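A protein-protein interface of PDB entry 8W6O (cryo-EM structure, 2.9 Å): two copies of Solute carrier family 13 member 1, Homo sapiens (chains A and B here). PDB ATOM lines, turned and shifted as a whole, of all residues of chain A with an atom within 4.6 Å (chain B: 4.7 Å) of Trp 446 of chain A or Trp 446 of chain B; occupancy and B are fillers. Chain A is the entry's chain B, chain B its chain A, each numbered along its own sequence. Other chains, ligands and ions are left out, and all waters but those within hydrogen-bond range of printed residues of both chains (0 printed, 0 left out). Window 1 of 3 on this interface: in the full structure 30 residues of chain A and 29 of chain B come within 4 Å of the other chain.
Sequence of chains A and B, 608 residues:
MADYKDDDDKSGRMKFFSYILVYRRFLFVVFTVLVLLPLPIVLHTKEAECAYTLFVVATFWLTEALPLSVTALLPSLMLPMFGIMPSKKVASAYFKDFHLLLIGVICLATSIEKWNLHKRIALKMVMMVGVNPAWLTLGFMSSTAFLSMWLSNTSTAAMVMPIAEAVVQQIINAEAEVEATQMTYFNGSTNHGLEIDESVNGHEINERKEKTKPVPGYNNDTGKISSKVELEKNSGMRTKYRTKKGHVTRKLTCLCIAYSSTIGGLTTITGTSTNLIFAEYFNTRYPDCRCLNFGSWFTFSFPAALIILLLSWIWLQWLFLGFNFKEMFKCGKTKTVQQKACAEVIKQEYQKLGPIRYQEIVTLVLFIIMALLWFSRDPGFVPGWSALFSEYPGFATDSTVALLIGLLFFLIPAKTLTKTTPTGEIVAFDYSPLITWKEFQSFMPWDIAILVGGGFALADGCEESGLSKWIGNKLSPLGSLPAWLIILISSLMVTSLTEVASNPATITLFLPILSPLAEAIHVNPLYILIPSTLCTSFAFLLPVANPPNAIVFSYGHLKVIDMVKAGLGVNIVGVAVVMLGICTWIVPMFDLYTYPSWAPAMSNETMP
Printed residues of chain B within 4 Å of Gln 441 of chain A: Gln 441 (3.6 Å), Met 444 (3.9 Å) and Trp 446 (3.3 Å).
Printed residues of chain B within 4 Å of Met 444 of chain A: Gln 441 (3.2 Å).
Printed residues of chain B within 4 Å of Trp 446 of chain A: Gln 441 (3.2 Å) and Trp 446 (3.7 Å).
Printed residues of chain A within 4 Å of Gln 441 of chain B: Gln 441 (3.6 Å), Met 444 (3.2 Å) and Trp 446 (3.2 Å).
Of the printed residues of chain A, Met 444 of chain B touches Gln 441 (3.9 Å).
The side-chain amide nitrogen of Gln 441 of chain B sits at hydrogen-bond distance from the backbone carbonyl oxygen of Met 444 of chain A.
Among the printed residues, pairs that only touch across the chains: Trp 446 of chain A with Gln 441 of chain B, Gln 441 of chain A with Trp 446 of chain B, Gln 441 of chain A with Gln 441 of chain B, Trp 446 of chain A with Trp 446 of chain B and Gln 441 of chain A with Met 444 of chain B.
Of the 8 printed residues of chain A, 3 touch a printed residue of chain B.
Printed residues of chain B that touch a printed residue of chain A: Gln 441, Met 444 and Trp 446.
Among the printed residues, 6 pairs touch across the chains.
Among the printed residues, no Asp or Glu carboxylate lies within 4 Å of a Lys or Arg side-chain nitrogen of the other chain.
Gln 441 of chain A touches its own counterpart, Gln 441 of chain B.
Gln 441 of chain A touches Met 444 of chain B, and with the chains exchanged Met 444 of chain A touches Gln 441 of chain B.
Gln 441 of chain A touches Trp 446 of chain B, and with the chains exchanged Trp 446 of chain A touches Gln 441 of chain B.
Trp 446 of chain B touches its own counterpart, Trp 446 of chain A.
Positions printed for both chains: 441, 444, 445, 446, 447, 448, 449 and 450.
Of the 6 pairs that touch across the chains among the printed residues, 6 have their exchanged pair printed and touching as well.
The indole nitrogen of Trp 446 of chain B is in hydrogen-bond range of the backbone carbonyl oxygen of Gln 441 of chain B, at 2.9 Å.
The indole nitrogen (NE1) of Trp 446 of chain B sits close to the backbone carbonyl oxygen (O) of Met 444 of chain B (3.5 Å).
The backbone carbonyl oxygen (O) of Gln 441 of chain A sits at hydrogen-bond distance from the indole nitrogen (NE1) of Trp 446 of chain A (3.1 Å).
The backbone carbonyl oxygen (O) of Met 444 of chain A lies close to the indole nitrogen (NE1) of Trp 446 of chain A (3.5 Å).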
ATOM      1  N   GLN A 441      -3.214  -1.852  22.137  1.00  0.00           N
ATOM      2  CA  GLN A 441      -2.849  -0.529  22.627  1.00  0.00           C
ATOM      3  C   GLN A 441      -3.422  -0.250  24.010  1.00  0.00           C
ATOM      4  O   GLN A 441      -2.835   0.529  24.767  1.00  0.00           O
ATOM      5  CB  GLN A 441      -3.326   0.532  21.637  1.00  0.00           C
ATOM      6  CG  GLN A 441      -2.549   1.828  21.666  1.00  0.00           C
ATOM      7  CD  GLN A 441      -3.039   2.810  20.626  1.00  0.00           C
ATOM      8  OE1 GLN A 441      -4.239   3.056  20.507  1.00  0.00           O
ATOM      9  NE2 GLN A 441      -2.114   3.372  19.859  1.00  0.00           N
ATOM     10  N   MET A 444      -0.985  -2.515  26.323  1.00  0.00           N
ATOM     11  CA  MET A 444       0.457  -2.285  26.272  1.00  0.00           C
ATOM     12  C   MET A 444       0.870  -1.214  27.276  1.00  0.00           C
ATOM     13  O   MET A 444       0.245  -0.152  27.331  1.00  0.00           O
ATOM     14  CB  MET A 444       0.886  -1.864  24.874  1.00  0.00           C
ATOM     15  CG  MET A 444       2.383  -1.722  24.703  1.00  0.00           C
ATOM     16  SD  MET A 444       3.217  -3.296  24.452  1.00  0.00           S
ATOM     17  CE  MET A 444       4.908  -2.743  24.302  1.00  0.00           C
ATOM     18  N   PRO A 445       1.904  -1.457  28.087  1.00  0.00           N
ATOM     19  CA  PRO A 445       2.439  -0.402  28.961  1.00  0.00           C
ATOM     20  C   PRO A 445       3.308   0.571  28.180  1.00  0.00           C
ATOM     21  O   PRO A 445       4.433   0.250  27.786  1.00  0.00           O
ATOM     22  CB  PRO A 445       3.249  -1.193  30.001  1.00  0.00           C
ATOM     23  CG  PRO A 445       3.586  -2.484  29.336  1.00  0.00           C
ATOM     24  CD  PRO A 445       2.470  -2.783  28.392  1.00  0.00           C
ATOM     25  N   TRP A 446       2.786   1.774  27.957  1.00  0.00           N
ATOM     26  CA  TRP A 446       3.537   2.793  27.239  1.00  0.00           C
ATOM     27  C   TRP A 446       4.273   3.753  28.163  1.00  0.00           C
ATOM     28  O   TRP A 446       5.274   4.346  27.747  1.00  0.00           O
ATOM     29  CB  TRP A 446       2.605   3.593  26.323  1.00  0.00           C
ATOM     30  CG  TRP A 446       1.787   2.767  25.373  1.00  0.00           C
ATOM     31  CD1 TRP A 446       0.460   2.481  25.477  1.00  0.00           C
ATOM     32  CD2 TRP A 446       2.234   2.154  24.159  1.00  0.00           C
ATOM     33  NE1 TRP A 446       0.053   1.714  24.414  1.00  0.00           N
ATOM     34  CE2 TRP A 446       1.123   1.502  23.588  1.00  0.00           C
ATOM     35  CE3 TRP A 446       3.465   2.087  23.502  1.00  0.00           C
ATOM     36  CZ2 TRP A 446       1.208   0.792  22.393  1.00  0.00           C
ATOM     37  CZ3 TRP A 446       3.546   1.381  22.315  1.00  0.00           C
ATOM     38  CH2 TRP A 446       2.424   0.742  21.774  1.00  0.00           C
ATOM     39  N   ASP A 447       3.809   3.913  29.402  1.00  0.00           N
ATOM     40  CA  ASP A 447       4.387   4.870  30.336  1.00  0.00           C
ATOM     41  C   ASP A 447       5.645   4.363  31.030  1.00  0.00           C
ATOM     42  O   ASP A 447       6.316   5.155  31.705  1.00  0.00           O
ATOM     43  CB  ASP A 447       3.345   5.254  31.386  1.00  0.00           C
ATOM     44  CG  ASP A 447       2.614   4.054  31.945  1.00  0.00           C
ATOM     45  OD1 ASP A 447       2.864   2.929  31.471  1.00  0.00           O
ATOM     46  OD2 ASP A 447       1.781   4.236  32.856  1.00  0.00           O
ATOM     47  N   ILE A 448       5.979   3.078  30.883  1.00  0.00           N
ATOM     48  CA  ILE A 448       7.172   2.530  31.522  1.00  0.00           C
ATOM     49  C   ILE A 448       8.431   3.097  30.872  1.00  0.00           C
ATOM     50  O   ILE A 448       9.414   3.416  31.558  1.00  0.00           O
ATOM     51  CB  ILE A 448       7.131   0.990  31.470  1.00  0.00           C
ATOM     52  CG1 ILE A 448       5.883   0.471  32.187  1.00  0.00           C
ATOM     53  CG2 ILE A 448       8.376   0.369  32.088  1.00  0.00           C
ATOM     54  CD1 ILE A 448       5.880   0.720  33.683  1.00  0.00           C
ATOM     55  N   ALA A 449       8.405   3.275  29.547  1.00  0.00           N
ATOM     56  CA  ALA A 449       9.535   3.883  28.851  1.00  0.00           C
ATOM     57  C   ALA A 449       9.680   5.356  29.209  1.00  0.00           C
ATOM     58  O   ALA A 449      10.801   5.866  29.315  1.00  0.00           O
ATOM     59  CB  ALA A 449       9.374   3.711  27.343  1.00  0.00           C
ATOM     60  N   ILE A 450       8.555   6.043  29.429  1.00  0.00           N
ATOM     61  CA  ILE A 450       8.584   7.426  29.894  1.00  0.00           C
ATOM     62  C   ILE A 450       9.177   7.507  31.297  1.00  0.00           C
ATOM     63  O   ILE A 450       9.950   8.423  31.607  1.00  0.00           O
ATOM     64  CB  ILE A 450       7.166   8.027  29.836  1.00  0.00           C
ATOM     65  CG1 ILE A 450       6.584   7.877  28.430  1.00  0.00           C
ATOM     66  CG2 ILE A 450       7.174   9.491  30.245  1.00  0.00           C
ATOM     67  CD1 ILE A 450       5.192   8.445  28.278  1.00  0.00           C
ATOM     68  N   GLN B 441      -3.833   8.026  26.938  1.00  0.00           N
ATOM     69  CA  GLN B 441      -3.226   6.843  26.338  1.00  0.00           C
ATOM     70  C   GLN B 441      -4.047   6.325  25.164  1.00  0.00           C
ATOM     71  O   GLN B 441      -3.489   5.755  24.221  1.00  0.00           O
ATOM     72  CB  GLN B 441      -3.070   5.764  27.408  1.00  0.00           C
ATOM     73  CG  GLN B 441      -2.190   4.592  27.034  1.00  0.00           C
ATOM     74  CD  GLN B 441      -2.218   3.506  28.087  1.00  0.00           C
ATOM     75  OE1 GLN B 441      -2.603   3.746  29.231  1.00  0.00           O
ATOM     76  NE2 GLN B 441      -1.819   2.300  27.706  1.00  0.00           N
ATOM     77  N   MET B 444      -3.336   9.093  22.286  1.00  0.00           N
ATOM     78  CA  MET B 444      -1.958   9.290  21.839  1.00  0.00           C
ATOM     79  C   MET B 444      -1.622   8.344  20.692  1.00  0.00           C
ATOM     80  O   MET B 444      -1.902   7.146  20.785  1.00  0.00           O
ATOM     81  CB  MET B 444      -0.984   9.067  22.986  1.00  0.00           C
ATOM     82  CG  MET B 444       0.462   9.342  22.635  1.00  0.00           C
ATOM     83  SD  MET B 444       0.876  11.092  22.666  1.00  0.00           S
ATOM     84  CE  MET B 444       2.606  11.023  22.229  1.00  0.00           C
ATOM     85  N   PRO B 445      -1.036   8.840  19.600  1.00  0.00           N
ATOM     86  CA  PRO B 445      -0.558   7.931  18.550  1.00  0.00           C
ATOM     87  C   PRO B 445       0.723   7.217  18.952  1.00  0.00           C
ATOM     88  O   PRO B 445       1.803   7.814  18.973  1.00  0.00           O
ATOM     89  CB  PRO B 445      -0.335   8.864  17.351  1.00  0.00           C
ATOM     90  CG  PRO B 445      -0.152  10.222  17.944  1.00  0.00           C
ATOM     91  CD  PRO B 445      -0.969  10.254  19.193  1.00  0.00           C
ATOM     92  N   TRP B 446       0.616   5.930  19.268  1.00  0.00           N
ATOM     93  CA  TRP B 446       1.785   5.153  19.656  1.00  0.00           C
ATOM     94  C   TRP B 446       2.402   4.392  18.491  1.00  0.00           C
ATOM     95  O   TRP B 446       3.600   4.090  18.533  1.00  0.00           O
ATOM     96  CB  TRP B 446       1.419   4.165  20.766  1.00  0.00           C
ATOM     97  CG  TRP B 446       0.795   4.786  21.981  1.00  0.00           C
ATOM     98  CD1 TRP B 446      -0.514   4.711  22.355  1.00  0.00           C
ATOM     99  CD2 TRP B 446       1.457   5.549  22.994  1.00  0.00           C
ATOM    100  NE1 TRP B 446      -0.711   5.392  23.530  1.00  0.00           N
ATOM    101  CE2 TRP B 446       0.485   5.913  23.944  1.00  0.00           C
ATOM    102  CE3 TRP B 446       2.777   5.965  23.186  1.00  0.00           C
ATOM    103  CZ2 TRP B 446       0.791   6.673  25.071  1.00  0.00           C
ATOM    104  CZ3 TRP B 446       3.078   6.720  24.306  1.00  0.00           C
ATOM    105  CH2 TRP B 446       2.088   7.068  25.233  1.00  0.00           C
ATOM    106  N   ASP B 447       1.622   4.090  17.456  1.00  0.00           N
ATOM    107  CA  ASP B 447       2.091   3.291  16.333  1.00  0.00           C
ATOM    108  C   ASP B 447       2.852   4.096  15.287  1.00  0.00           C
ATOM    109  O   ASP B 447       3.429   3.493  14.376  1.00  0.00           O
ATOM    110  CB  ASP B 447       0.908   2.586  15.672  1.00  0.00           C
ATOM    111  CG  ASP B 447      -0.277   3.503  15.473  1.00  0.00           C
ATOM    112  OD1 ASP B 447      -0.207   4.671  15.905  1.00  0.00           O
ATOM    113  OD2 ASP B 447      -1.284   3.055  14.890  1.00  0.00           O
ATOM    114  N   ILE B 448       2.867   5.428  15.391  1.00  0.00           N
ATOM    115  CA  ILE B 448       3.609   6.246  14.435  1.00  0.00           C
ATOM    116  C   ILE B 448       5.111   6.066  14.638  1.00  0.00           C
ATOM    117  O   ILE B 448       5.885   6.009  13.669  1.00  0.00           O
ATOM    118  CB  ILE B 448       3.174   7.719  14.563  1.00  0.00           C
ATOM    119  CG1 ILE B 448       1.674   7.851  14.293  1.00  0.00           C
ATOM    120  CG2 ILE B 448       3.943   8.623  13.608  1.00  0.00           C
ATOM    121  CD1 ILE B 448       1.268   7.503  12.875  1.00  0.00           C
ATOM    122  N   ALA B 449       5.540   5.924  15.897  1.00  0.00           N
ATOM    123  CA  ALA B 449       6.948   5.672  16.187  1.00  0.00           C
ATOM    124  C   ALA B 449       7.370   4.286  15.720  1.00  0.00           C
ATOM    125  O   ALA B 449       8.484   4.109  15.215  1.00  0.00           O
ATOM    126  CB  ALA B 449       7.212   5.841  17.682  1.00  0.00           C
ATOM    127  N   ILE B 450       6.478   3.300  15.851  1.00  0.00           N
ATOM    128  CA  ILE B 450       6.747   1.958  15.343  1.00  0.00           C
ATOM    129  C   ILE B 450       6.827   1.969  13.820  1.00  0.00           C
ATOM    130  O   ILE B 450       7.680   1.296  13.224  1.00  0.00           O
ATOM    131  CB  ILE B 450       5.671   0.982  15.854  1.00  0.00           C
ATOM    132  CG1 ILE B 450       5.595   1.030  17.381  1.00  0.00           C
ATOM    133  CG2 ILE B 450       5.950  -0.436  15.390  1.00  0.00           C
ATOM    134  CD1 ILE B 450       4.537   0.127  17.968  1.00  0.00           C
